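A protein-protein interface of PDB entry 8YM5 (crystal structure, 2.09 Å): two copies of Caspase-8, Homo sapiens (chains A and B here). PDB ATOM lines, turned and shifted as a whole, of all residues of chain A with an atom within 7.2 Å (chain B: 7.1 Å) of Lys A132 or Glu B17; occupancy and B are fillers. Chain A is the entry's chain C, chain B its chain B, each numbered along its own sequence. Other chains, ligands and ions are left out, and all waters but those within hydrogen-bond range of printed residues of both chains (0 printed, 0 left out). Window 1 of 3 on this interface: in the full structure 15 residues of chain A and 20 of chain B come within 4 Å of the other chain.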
ATOM      1  N   GLU A  36      26.361  15.124 -15.742  1.00  0.00           N
ATOM      2  CA  GLU A  36      26.715  13.833 -15.153  1.00  0.00           C
ATOM      3  C   GLU A  36      28.210  13.494 -15.193  1.00  0.00           C
ATOM      4  O   GLU A  36      28.750  13.089 -14.154  1.00  0.00           O
ATOM      5  CB  GLU A  36      25.899  12.732 -15.842  1.00  0.00           C
ATOM      6  CG  GLU A  36      26.113  11.368 -15.243  1.00  0.00           C
ATOM      7  CD  GLU A  36      25.155  10.341 -15.816  1.00  0.00           C
ATOM      8  OE1 GLU A  36      24.664  10.553 -16.946  1.00  0.00           O
ATOM      9  OE2 GLU A  36      24.902   9.319 -15.144  1.00  0.00           O
ATOM     10  N   LYS A 121      14.552  15.479   4.340  1.00  0.00           N
ATOM     11  CA  LYS A 121      14.118  14.325   3.565  1.00  0.00           C
ATOM     12  C   LYS A 121      12.864  13.709   4.174  1.00  0.00           C
ATOM     13  O   LYS A 121      11.949  13.294   3.449  1.00  0.00           O
ATOM     14  CB  LYS A 121      15.248  13.296   3.491  1.00  0.00           C
ATOM     15  CG  LYS A 121      16.372  13.650   2.528  1.00  0.00           C
ATOM     16  CD  LYS A 121      17.583  12.756   2.780  1.00  0.00           C
ATOM     17  CE  LYS A 121      18.756  13.151   1.910  1.00  0.00           C
ATOM     18  NZ  LYS A 121      20.004  12.367   2.228  1.00  0.00           N
ATOM     19  N   LEU A 124       9.813  15.506   3.043  1.00  0.00           N
ATOM     20  CA  LEU A 124       9.385  15.350   1.650  1.00  0.00           C
ATOM     21  C   LEU A 124       8.800  13.973   1.303  1.00  0.00           C
ATOM     22  O   LEU A 124       8.626  13.682   0.114  1.00  0.00           O
ATOM     23  CB  LEU A 124      10.556  15.644   0.711  1.00  0.00           C
ATOM     24  CG  LEU A 124      10.956  17.113   0.691  1.00  0.00           C
ATOM     25  CD1 LEU A 124      12.314  17.234   0.017  1.00  0.00           C
ATOM     26  CD2 LEU A 124       9.929  17.941  -0.030  1.00  0.00           C
ATOM     27  N   ILE A 128       8.407  13.042  -2.885  1.00  0.00           N
ATOM     28  CA  ILE A 128       9.530  12.444  -3.596  1.00  0.00           C
ATOM     29  C   ILE A 128       9.587  10.952  -3.289  1.00  0.00           C
ATOM     30  O   ILE A 128       9.347  10.534  -2.151  1.00  0.00           O
ATOM     31  CB  ILE A 128      10.839  13.160  -3.213  1.00  0.00           C
ATOM     32  CG1 ILE A 128      10.730  14.637  -3.607  1.00  0.00           C
ATOM     33  CG2 ILE A 128      12.041  12.491  -3.859  1.00  0.00           C
ATOM     34  CD1 ILE A 128      11.930  15.447  -3.196  1.00  0.00           C
ATOM     35  N   SER A 129       9.900  10.149  -4.311  1.00  0.00           N
ATOM     36  CA  SER A 129      10.041   8.708  -4.126  1.00  0.00           C
ATOM     37  C   SER A 129      11.184   8.388  -3.162  1.00  0.00           C
ATOM     38  O   SER A 129      12.160   9.135  -3.047  1.00  0.00           O
ATOM     39  CB  SER A 129      10.296   8.021  -5.464  1.00  0.00           C
ATOM     40  OG  SER A 129      11.414   8.598  -6.115  1.00  0.00           O
ATOM     41  N   LYS A 130      11.057   7.242  -2.485  1.00  0.00           N
ATOM     42  CA  LYS A 130      11.990   6.889  -1.416  1.00  0.00           C
ATOM     43  C   LYS A 130      13.424   6.764  -1.928  1.00  0.00           C
ATOM     44  O   LYS A 130      14.369   7.183  -1.252  1.00  0.00           O
ATOM     45  CB  LYS A 130      11.542   5.585  -0.752  1.00  0.00           C
ATOM     46  CG  LYS A 130      12.400   5.150   0.433  1.00  0.00           C
ATOM     47  CD  LYS A 130      11.686   4.099   1.282  1.00  0.00           C
ATOM     48  CE  LYS A 130      10.203   4.398   1.398  1.00  0.00           C
ATOM     49  NZ  LYS A 130       9.379   3.156   1.400  1.00  0.00           N
ATOM     50  N   CYS A 131      13.613   6.179  -3.115  1.00  0.00           N
ATOM     51  CA  CYS A 131      14.965   6.027  -3.647  1.00  0.00           C
ATOM     52  C   CYS A 131      15.633   7.376  -3.905  1.00  0.00           C
ATOM     53  O   CYS A 131      16.864   7.473  -3.834  1.00  0.00           O
ATOM     54  CB  CYS A 131      14.935   5.154  -4.907  1.00  0.00           C
ATOM     55  SG  CYS A 131      14.572   6.053  -6.440  1.00  0.00           S
ATOM     56  N   LYS A 132      14.857   8.432  -4.162  1.00  0.00           N
ATOM     57  CA  LYS A 132      15.427   9.765  -4.324  1.00  0.00           C
ATOM     58  C   LYS A 132      15.497  10.536  -3.005  1.00  0.00           C
ATOM     59  O   LYS A 132      15.706  11.752  -3.019  1.00  0.00           O
ATOM     60  CB  LYS A 132      14.640  10.564  -5.371  1.00  0.00           C
ATOM     61  CG  LYS A 132      14.875  10.099  -6.822  1.00  0.00           C
ATOM     62  CD  LYS A 132      16.086  10.823  -7.459  1.00  0.00           C
ATOM     63  CE  LYS A 132      16.354  10.377  -8.906  1.00  0.00           C
ATOM     64  NZ  LYS A 132      15.522  11.073  -9.958  1.00  0.00           N
ATOM     65  N   LEU A 133      15.308   9.854  -1.873  1.00  0.00           N
ATOM     66  CA  LEU A 133      15.545  10.415  -0.547  1.00  0.00           C
ATOM     67  C   LEU A 133      16.621   9.633   0.197  1.00  0.00           C
ATOM     68  O   LEU A 133      16.707   9.708   1.426  1.00  0.00           O
ATOM     69  CB  LEU A 133      14.253  10.449   0.268  1.00  0.00           C
ATOM     70  CG  LEU A 133      13.140  11.306  -0.328  1.00  0.00           C
ATOM     71  CD1 LEU A 133      11.855  11.165   0.482  1.00  0.00           C
ATOM     72  CD2 LEU A 133      13.579  12.758  -0.423  1.00  0.00           C
ATOM     73  N   ASP A 134      17.430   8.878  -0.533  1.00  0.00           N
ATOM     74  CA  ASP A 134      18.448   8.023   0.049  1.00  0.00           C
ATOM     75  C   ASP A 134      19.483   8.848   0.809  1.00  0.00           C
ATOM     76  O   ASP A 134      19.656  10.049   0.584  1.00  0.00           O
ATOM     77  CB  ASP A 134      19.120   7.193  -1.047  1.00  0.00           C
ATOM     78  CG  ASP A 134      19.627   5.857  -0.539  1.00  0.00           C
ATOM     79  OD1 ASP A 134      18.835   4.884  -0.520  1.00  0.00           O
ATOM     80  OD2 ASP A 134      20.824   5.782  -0.171  1.00  0.00           O
ATOM     81  N   ASP A 135      20.190   8.173   1.715  1.00  0.00           N
ATOM     82  CA  ASP A 135      21.045   8.862   2.674  1.00  0.00           C
ATOM     83  C   ASP A 135      22.231   9.564   2.020  1.00  0.00           C
ATOM     84  O   ASP A 135      22.715  10.561   2.566  1.00  0.00           O
ATOM     85  CB  ASP A 135      21.528   7.854   3.717  1.00  0.00           C
ATOM     86  CG  ASP A 135      20.389   7.020   4.284  1.00  0.00           C
ATOM     87  OD1 ASP A 135      19.309   7.592   4.539  1.00  0.00           O
ATOM     88  OD2 ASP A 135      20.563   5.794   4.454  1.00  0.00           O
ATOM     89  N   MET A 137      22.118  11.258  -0.865  1.00  0.00           N
ATOM     90  CA  MET A 137      21.679  12.502  -1.504  1.00  0.00           C
ATOM     91  C   MET A 137      22.015  13.725  -0.638  1.00  0.00           C
ATOM     92  O   MET A 137      21.723  13.736   0.554  1.00  0.00           O
ATOM     93  CB  MET A 137      20.167  12.472  -1.778  1.00  0.00           C
ATOM     94  CG  MET A 137      19.676  11.276  -2.595  1.00  0.00           C
ATOM     95  SD  MET A 137      19.749  11.659  -4.509  1.00  0.00           S
ATOM     96  CE  MET A 137      18.237  12.922  -4.583  1.00  0.00           C
ATOM     97  N   ASN A 138      22.637  14.748  -1.225  1.00  0.00           N
ATOM     98  CA  ASN A 138      22.793  16.012  -0.523  1.00  0.00           C
ATOM     99  C   ASN A 138      21.578  16.902  -0.810  1.00  0.00           C
ATOM    100  O   ASN A 138      20.658  16.527  -1.541  1.00  0.00           O
ATOM    101  CB  ASN A 138      24.135  16.681  -0.873  1.00  0.00           C
ATOM    102  CG  ASN A 138      24.301  17.003  -2.363  1.00  0.00           C
ATOM    103  OD1 ASN A 138      23.363  17.428  -3.034  1.00  0.00           O
ATOM    104  ND2 ASN A 138      25.531  16.824  -2.878  1.00  0.00           N
ATOM    105  N   ASP A 141      20.997  17.944  -4.534  1.00  0.00           N
ATOM    106  CA  ASP A 141      20.387  16.870  -5.329  1.00  0.00           C
ATOM    107  C   ASP A 141      18.882  16.815  -5.098  1.00  0.00           C
ATOM    108  O   ASP A 141      18.104  16.574  -6.027  1.00  0.00           O
ATOM    109  CB  ASP A 141      20.972  15.512  -4.944  1.00  0.00           C
ATOM    110  CG  ASP A 141      22.454  15.394  -5.224  1.00  0.00           C
ATOM    111  OD1 ASP A 141      22.895  15.895  -6.278  1.00  0.00           O
ATOM    112  OD2 ASP A 141      23.165  14.787  -4.385  1.00  0.00           O
ATOM    113  N   ILE A 142      18.469  16.985  -3.848  1.00  0.00           N
ATOM    114  CA  ILE A 142      17.045  17.015  -3.514  1.00  0.00           C
ATOM    115  C   ILE A 142      16.343  18.171  -4.227  1.00  0.00           C
ATOM    116  O   ILE A 142      15.225  18.019  -4.757  1.00  0.00           O
ATOM    117  CB  ILE A 142      16.885  17.108  -1.987  1.00  0.00           C
ATOM    118  CG1 ILE A 142      17.464  15.856  -1.311  1.00  0.00           C
ATOM    119  CG2 ILE A 142      15.397  17.347  -1.599  1.00  0.00           C
ATOM    120  CD1 ILE A 142      16.743  14.572  -1.654  1.00  0.00           C
ATOM    121  N   GLU A 145      15.750  17.297  -7.747  1.00  0.00           N
ATOM    122  CA  GLU A 145      14.633  16.367  -7.890  1.00  0.00           C
ATOM    123  C   GLU A 145      13.284  17.083  -7.755  1.00  0.00           C
ATOM    124  O   GLU A 145      12.335  16.781  -8.483  1.00  0.00           O
ATOM    125  CB  GLU A 145      14.784  15.247  -6.862  1.00  0.00           C
ATOM    126  CG  GLU A 145      13.683  14.185  -6.899  1.00  0.00           C
ATOM    127  CD  GLU A 145      13.504  13.590  -8.288  1.00  0.00           C
ATOM    128  OE1 GLU A 145      12.352  13.600  -8.796  1.00  0.00           O
ATOM    129  OE2 GLU A 145      14.535  13.190  -8.888  1.00  0.00           O
ATOM    130  N   LYS A 148      12.543  18.883 -10.975  1.00  0.00           N
ATOM    131  CA  LYS A 148      12.085  17.970 -12.015  1.00  0.00           C
ATOM    132  C   LYS A 148      10.617  17.650 -11.863  1.00  0.00           C
ATOM    133  O   LYS A 148       9.914  17.429 -12.864  1.00  0.00           O
ATOM    134  CB  LYS A 148      12.886  16.671 -11.973  1.00  0.00           C
ATOM    135  CG  LYS A 148      14.288  16.809 -12.473  1.00  0.00           C
ATOM    136  CD  LYS A 148      15.051  15.509 -12.214  1.00  0.00           C
ATOM    137  CE  LYS A 148      16.486  15.627 -12.748  1.00  0.00           C
ATOM    138  NZ  LYS A 148      17.320  14.454 -12.332  1.00  0.00           N
ATOM    139  N   ARG A 149      10.144  17.572 -10.625  1.00  0.00           N
ATOM    140  CA  ARG A 149       8.739  17.310 -10.391  1.00  0.00           C
ATOM    141  C   ARG A 149       7.935  18.592 -10.338  1.00  0.00           C
ATOM    142  O   ARG A 149       6.736  18.532 -10.075  1.00  0.00           O
ATOM    143  CB  ARG A 149       8.552  16.533  -9.093  1.00  0.00           C
ATOM    144  CG  ARG A 149       9.050  15.127  -9.152  1.00  0.00           C
ATOM    145  CD  ARG A 149       9.151  14.585  -7.741  1.00  0.00           C
ATOM    146  NE  ARG A 149       9.892  13.333  -7.705  1.00  0.00           N
ATOM    147  CZ  ARG A 149       9.323  12.140  -7.618  1.00  0.00           C
ATOM    148  NH1 ARG A 149       8.009  12.008  -7.539  1.00  0.00           N
ATOM    149  NH2 ARG A 149      10.093  11.054  -7.609  1.00  0.00           N
ATOM    150  N   LEU B  14      18.405  14.623 -20.151  1.00  0.00           N
ATOM    151  CA  LEU B  14      18.189  13.270 -19.643  1.00  0.00           C
ATOM    152  C   LEU B  14      19.540  12.584 -19.461  1.00  0.00           C
ATOM    153  O   LEU B  14      20.280  12.402 -20.436  1.00  0.00           O
ATOM    154  CB  LEU B  14      17.325  12.456 -20.620  1.00  0.00           C
ATOM    155  CG  LEU B  14      15.876  12.892 -20.814  1.00  0.00           C
ATOM    156  CD1 LEU B  14      15.237  12.265 -22.104  1.00  0.00           C
ATOM    157  CD2 LEU B  14      15.052  12.553 -19.554  1.00  0.00           C
ATOM    158  N   ASP B  15      19.859  12.179 -18.233  1.00  0.00           N
ATOM    159  CA  ASP B  15      21.144  11.536 -17.986  1.00  0.00           C
ATOM    160  C   ASP B  15      20.974  10.012 -18.058  1.00  0.00           C
ATOM    161  O   ASP B  15      19.934   9.497 -18.487  1.00  0.00           O
ATOM    162  CB  ASP B  15      21.753  12.052 -16.681  1.00  0.00           C
ATOM    163  CG  ASP B  15      20.945  11.697 -15.430  1.00  0.00           C
ATOM    164  OD1 ASP B  15      20.198  10.688 -15.388  1.00  0.00           O
ATOM    165  OD2 ASP B  15      21.069  12.468 -14.460  1.00  0.00           O
ATOM    166  N   SER B  16      22.002   9.269 -17.649  1.00  0.00           N
ATOM    167  CA  SER B  16      22.000   7.827 -17.879  1.00  0.00           C
ATOM    168  C   SER B  16      20.988   7.088 -17.001  1.00  0.00           C
ATOM    169  O   SER B  16      20.503   6.027 -17.401  1.00  0.00           O
ATOM    170  CB  SER B  16      23.416   7.264 -17.678  1.00  0.00           C
ATOM    171  OG  SER B  16      23.774   7.283 -16.321  1.00  0.00           O
ATOM    172  N   GLU B  17      20.691   7.590 -15.796  1.00  0.00           N
ATOM    173  CA  GLU B  17      19.641   6.983 -14.968  1.00  0.00           C
ATOM    174  C   GLU B  17      18.245   7.194 -15.559  1.00  0.00           C
ATOM    175  O   GLU B  17      17.449   6.247 -15.647  1.00  0.00           O
ATOM    176  CB  GLU B  17      19.703   7.533 -13.541  1.00  0.00           C
ATOM    177  CG  GLU B  17      18.461   7.180 -12.707  1.00  0.00           C
ATOM    178  CD  GLU B  17      18.619   7.480 -11.216  1.00  0.00           C
ATOM    179  OE1 GLU B  17      18.360   6.569 -10.393  1.00  0.00           O
ATOM    180  OE2 GLU B  17      19.000   8.622 -10.867  1.00  0.00           O
ATOM    181  N   ASP B  18      17.918   8.436 -15.947  1.00  0.00           N
ATOM    182  CA  ASP B  18      16.651   8.692 -16.641  1.00  0.00           C
ATOM    183  C   ASP B  18      16.538   7.813 -17.878  1.00  0.00           C
ATOM    184  O   ASP B  18      15.465   7.278 -18.185  1.00  0.00           O
ATOM    185  CB  ASP B  18      16.535  10.182 -16.996  1.00  0.00           C
ATOM    186  CG  ASP B  18      16.025  11.020 -15.814  1.00  0.00           C
ATOM    187  OD1 ASP B  18      15.877  10.434 -14.726  1.00  0.00           O
ATOM    188  OD2 ASP B  18      15.806  12.254 -15.940  1.00  0.00           O
ATOM    189  N   LEU B  19      17.646   7.649 -18.602  1.00  0.00           N
ATOM    190  CA  LEU B  19      17.641   6.822 -19.796  1.00  0.00           C
ATOM    191  C   LEU B  19      17.357   5.369 -19.456  1.00  0.00           C
ATOM    192  O   LEU B  19      16.583   4.705 -20.156  1.00  0.00           O
ATOM    193  CB  LEU B  19      18.996   6.927 -20.511  1.00  0.00           C
ATOM    194  CG  LEU B  19      19.096   6.071 -21.785  1.00  0.00           C
ATOM    195  CD1 LEU B  19      18.134   6.601 -22.846  1.00  0.00           C
ATOM    196  CD2 LEU B  19      20.538   5.997 -22.322  1.00  0.00           C
ATOM    197  N   ALA B  20      18.003   4.842 -18.410  1.00  0.00           N
ATOM    198  CA  ALA B  20      17.715   3.471 -18.005  1.00  0.00           C
ATOM    199  C   ALA B  20      16.226   3.298 -17.686  1.00  0.00           C
ATOM    200  O   ALA B  20      15.617   2.277 -18.033  1.00  0.00           O
ATOM    201  CB  ALA B  20      18.591   3.082 -16.812  1.00  0.00           C
ATOM    202  N   SER B  21      15.629   4.293 -17.022  1.00  0.00           N
ATOM    203  CA  SER B  21      14.192   4.245 -16.738  1.00  0.00           C
ATOM    204  C   SER B  21      13.369   4.257 -18.019  1.00  0.00           C
ATOM    205  O   SER B  21      12.404   3.502 -18.153  1.00  0.00           O
ATOM    206  CB  SER B  21      13.796   5.420 -15.842  1.00  0.00           C
ATOM    207  OG  SER B  21      14.440   5.296 -14.600  1.00  0.00           O
ATOM    208  N   LEU B  22      13.721   5.142 -18.960  1.00  0.00           N
ATOM    209  CA  LEU B  22      12.986   5.236 -20.224  1.00  0.00           C
ATOM    210  C   LEU B  22      13.054   3.930 -21.003  1.00  0.00           C
ATOM    211  O   LEU B  22      12.057   3.476 -21.578  1.00  0.00           O
ATOM    212  CB  LEU B  22      13.559   6.373 -21.075  1.00  0.00           C
ATOM    213  CG  LEU B  22      13.278   7.768 -20.516  1.00  0.00           C
ATOM    214  CD1 LEU B  22      14.019   8.830 -21.326  1.00  0.00           C
ATOM    215  CD2 LEU B  22      11.753   8.021 -20.499  1.00  0.00           C
ATOM    216  N   LYS B  23      14.223   3.311 -21.027  1.00  0.00           N
ATOM    217  CA  LYS B  23      14.387   2.046 -21.730  1.00  0.00           C
ATOM    218  C   LYS B  23      13.569   0.947 -21.069  1.00  0.00           C
ATOM    219  O   LYS B  23      12.971   0.115 -21.758  1.00  0.00           O
ATOM    220  CB  LYS B  23      15.875   1.678 -21.778  1.00  0.00           C
ATOM    221  CG  LYS B  23      16.674   2.503 -22.785  1.00  0.00           C
ATOM    222  CD  LYS B  23      18.202   2.350 -22.583  1.00  0.00           C
ATOM    223  CE  LYS B  23      18.662   0.906 -22.681  1.00  0.00           C
ATOM    224  NZ  LYS B  23      20.173   0.834 -22.658  1.00  0.00           N
ATOM    225  N   ILE B  69       8.338   8.943 -15.753  1.00  0.00           N
ATOM    226  CA  ILE B  69       9.600   9.097 -15.013  1.00  0.00           C
ATOM    227  C   ILE B  69       9.651  10.419 -14.254  1.00  0.00           C
ATOM    228  O   ILE B  69      10.710  10.806 -13.766  1.00  0.00           O
ATOM    229  CB  ILE B  69      10.847   8.932 -15.915  1.00  0.00           C
ATOM    230  CG1 ILE B  69      10.956  10.022 -16.990  1.00  0.00           C
ATOM    231  CG2 ILE B  69      10.861   7.562 -16.598  1.00  0.00           C
ATOM    232  CD1 ILE B  69      12.409  10.145 -17.572  1.00  0.00           C
ATOM    233  N   ARG B  71       9.427  13.579 -15.039  1.00  0.00           N
ATOM    234  CA  ARG B  71      10.093  14.742 -15.626  1.00  0.00           C
ATOM    235  C   ARG B  71       9.053  15.768 -16.082  1.00  0.00           C
ATOM    236  O   ARG B  71       8.881  16.060 -17.272  1.00  0.00           O
ATOM    237  CB  ARG B  71      10.993  14.305 -16.774  1.00  0.00           C
ATOM    238  CG  ARG B  71      12.256  13.497 -16.340  1.00  0.00           C
ATOM    239  CD  ARG B  71      13.053  14.184 -15.213  1.00  0.00           C
ATOM    240  NE  ARG B  71      13.621  15.458 -15.650  1.00  0.00           N
ATOM    241  CZ  ARG B  71      14.840  15.597 -16.160  1.00  0.00           C
ATOM    242  NH1 ARG B  71      15.643  14.551 -16.326  1.00  0.00           N
ATOM    243  NH2 ARG B  71      15.264  16.810 -16.509  1.00  0.00           N
ATOM    244  N   TYR B 106       7.987  -0.245 -12.334  1.00  0.00           N
ATOM    245  CA  TYR B 106       8.825   0.947 -12.201  1.00  0.00           C
ATOM    246  C   TYR B 106       8.558   1.673 -10.875  1.00  0.00           C
ATOM    247  O   TYR B 106       9.497   2.139 -10.213  1.00  0.00           O
ATOM    248  CB  TYR B 106       8.627   1.891 -13.405  1.00  0.00           C
ATOM    249  CG  TYR B 106       9.425   3.192 -13.287  1.00  0.00           C
ATOM    250  CD1 TYR B 106      10.809   3.221 -13.477  1.00  0.00           C
ATOM    251  CD2 TYR B 106       8.795   4.379 -12.932  1.00  0.00           C
ATOM    252  CE1 TYR B 106      11.542   4.420 -13.324  1.00  0.00           C
ATOM    253  CE2 TYR B 106       9.509   5.569 -12.781  1.00  0.00           C
ATOM    254  CZ  TYR B 106      10.873   5.584 -12.984  1.00  0.00           C
ATOM    255  OH  TYR B 106      11.542   6.773 -12.831  1.00  0.00           O
ATOM    256  N   GLU B 110      11.024   2.607  -7.764  1.00  0.00           N
ATOM    257  CA  GLU B 110      11.180   3.947  -7.221  1.00  0.00           C
ATOM    258  C   GLU B 110      11.075   3.956  -5.702  1.00  0.00           C
ATOM    259  O   GLU B 110      11.621   4.856  -5.053  1.00  0.00           O
ATOM    260  CB  GLU B 110      10.139   4.887  -7.828  1.00  0.00           C
ATOM    261  CG  GLU B 110      10.499   5.387  -9.231  1.00  0.00           C
ATOM    262  CD  GLU B 110      11.879   6.052  -9.298  1.00  0.00           C
ATOM    263  OE1 GLU B 110      12.841   5.408  -9.782  1.00  0.00           O
ATOM    264  OE2 GLU B 110      12.003   7.222  -8.867  1.00  0.00           O
ATOM    265  N   GLU B 111      10.399   2.976  -5.109  1.00  0.00           N
ATOM    266  CA  GLU B 111      10.252   2.996  -3.662  1.00  0.00           C
ATOM    267  C   GLU B 111      11.269   2.141  -2.900  1.00  0.00           C
ATOM    268  O   GLU B 111      11.255   2.160  -1.669  1.00  0.00           O
ATOM    269  CB  GLU B 111       8.826   2.590  -3.282  1.00  0.00           C
ATOM    270  CG  GLU B 111       7.807   3.665  -3.669  1.00  0.00           C
ATOM    271  CD  GLU B 111       8.067   4.996  -2.961  1.00  0.00           C
ATOM    272  OE1 GLU B 111       8.088   5.005  -1.714  1.00  0.00           O
ATOM    273  OE2 GLU B 111       8.253   6.029  -3.647  1.00  0.00           O
ATOM    274  N   VAL B 112      12.168   1.427  -3.572  1.00  0.00           N
ATOM    275  CA  VAL B 112      13.100   0.527  -2.891  1.00  0.00           C
ATOM    276  C   VAL B 112      14.451   1.225  -2.730  1.00  0.00           C
ATOM    277  O   VAL B 112      15.074   1.632  -3.719  1.00  0.00           O
ATOM    278  CB  VAL B 112      13.252  -0.797  -3.656  1.00  0.00           C
ATOM    279  CG1 VAL B 112      14.382  -1.619  -3.072  1.00  0.00           C
ATOM    280  CG2 VAL B 112      11.944  -1.580  -3.621  1.00  0.00           C
ATOM    281  N   ASN B 138      20.566  -3.110 -10.356  1.00  0.00           N
ATOM    282  CA  ASN B 138      19.476  -2.387  -9.718  1.00  0.00           C
ATOM    283  C   ASN B 138      18.193  -3.227  -9.793  1.00  0.00           C
ATOM    284  O   ASN B 138      18.162  -4.302 -10.403  1.00  0.00           O
ATOM    285  CB  ASN B 138      19.302  -1.006 -10.357  1.00  0.00           C
ATOM    286  CG  ASN B 138      18.993  -1.078 -11.845  1.00  0.00           C
ATOM    287  OD1 ASN B 138      18.452  -2.069 -12.332  1.00  0.00           O
ATOM    288  ND2 ASN B 138      19.327  -0.019 -12.571  1.00  0.00           N
ATOM    289  N   LEU B 140      15.326  -2.800 -11.387  1.00  0.00           N
ATOM    290  CA  LEU B 140      14.770  -3.021 -12.725  1.00  0.00           C
ATOM    291  C   LEU B 140      15.466  -4.178 -13.446  1.00  0.00           C
ATOM    292  O   LEU B 140      14.807  -4.995 -14.101  1.00  0.00           O
ATOM    293  CB  LEU B 140      14.859  -1.735 -13.548  1.00  0.00           C
ATOM    294  CG  LEU B 140      14.012  -0.587 -12.970  1.00  0.00           C
ATOM    295  CD1 LEU B 140      14.189   0.674 -13.792  1.00  0.00           C
ATOM    296  CD2 LEU B 140      12.527  -0.986 -12.856  1.00  0.00           C
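The side-chain hydroxyl of Ser A129 is in hydrogen-bond range of the side-chain carboxylate of Glu B110, at 3.1 Å. The side-chain amino group of Lys A130 is in salt-bridge range of the side-chain carboxylate of Glu B111 (3.8 Å). OE2 of Glu A36 lies within hydrogen-bond range of OG of Ser B16. The backbone NH (N) of Cys A131 is in hydrogen-bond range of the backbone carbonyl oxygen (O) of Glu B110, 3.1 Å away.
The side-chain hydroxyl of Ser A129 sits at hydrogen-bond distance from the guanidinium group of Arg A149 (3.2 Å). The side-chain carboxylate (OD2) of Asp B18 is in salt-bridge range of the guanidinium group (NE) of Arg B71, 3.9 Å away. The side-chain hydroxyl (OG) of Ser B21 is in hydrogen-bond range of the backbone carbonyl oxygen (O) of Glu B17, 3.3 Å away. OE2 of Glu A145 is in salt-bridge range of NZ of Lys A132 (2.6 Å). The side-chain carboxylate (OD1) of Asp B15 sits at hydrogen-bond distance from the backbone NH (N) of Glu B17. N of Asp B18 sits at hydrogen-bond distance from OD1 of Asp B15 (3.3 Å).
Asp B15 touches Glu A36. OE2 of Glu B111 touches CA of Ser A129 (3.3 Å). O of Glu B110 touches N of Lys A130, at 3.6 Å. Cys A131 touches Val B112. OE2 of Glu B17 touches CE of Lys A132, 3.7 Å away. CG of Lys A148 touches NE of Arg B71, 3.5 Å away.
Of chain B, only Glu B17 comes within 4 Å of Lys A132. Of chain A, only Lys A132 comes within 4 Å of Glu B17. Printed residues of chain B within 4 Å of Lys A130: Glu B110 and Glu B111. Of the printed residues of chain B, Ser A129 touches Glu B110 and Glu B111. Of the printed residues of chain A, Glu B111 touches Ser A129 (3.3 Å) and Lys A130 (3.3 Å). Asp A141 touches none of the printed residues of chain B. The nearest residue of chain A that does not touch Glu B17 is Glu A36 (4.6 Å). The nearest printed residue of chain B that does not touch Glu A36 is Glu B17 (4.6 Å).
Printed residues of chain A that touch a printed residue of chain B: Glu A36, Ser A129, Lys A130, Cys A131, Lys A132 and Lys A148. Among the printed residues, 10 pairs touch across the chains.
1 position is printed for both chains. Of the 10 pairs that touch across the chains among the printed residues, none has its exchanged pair printed and touching as well.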
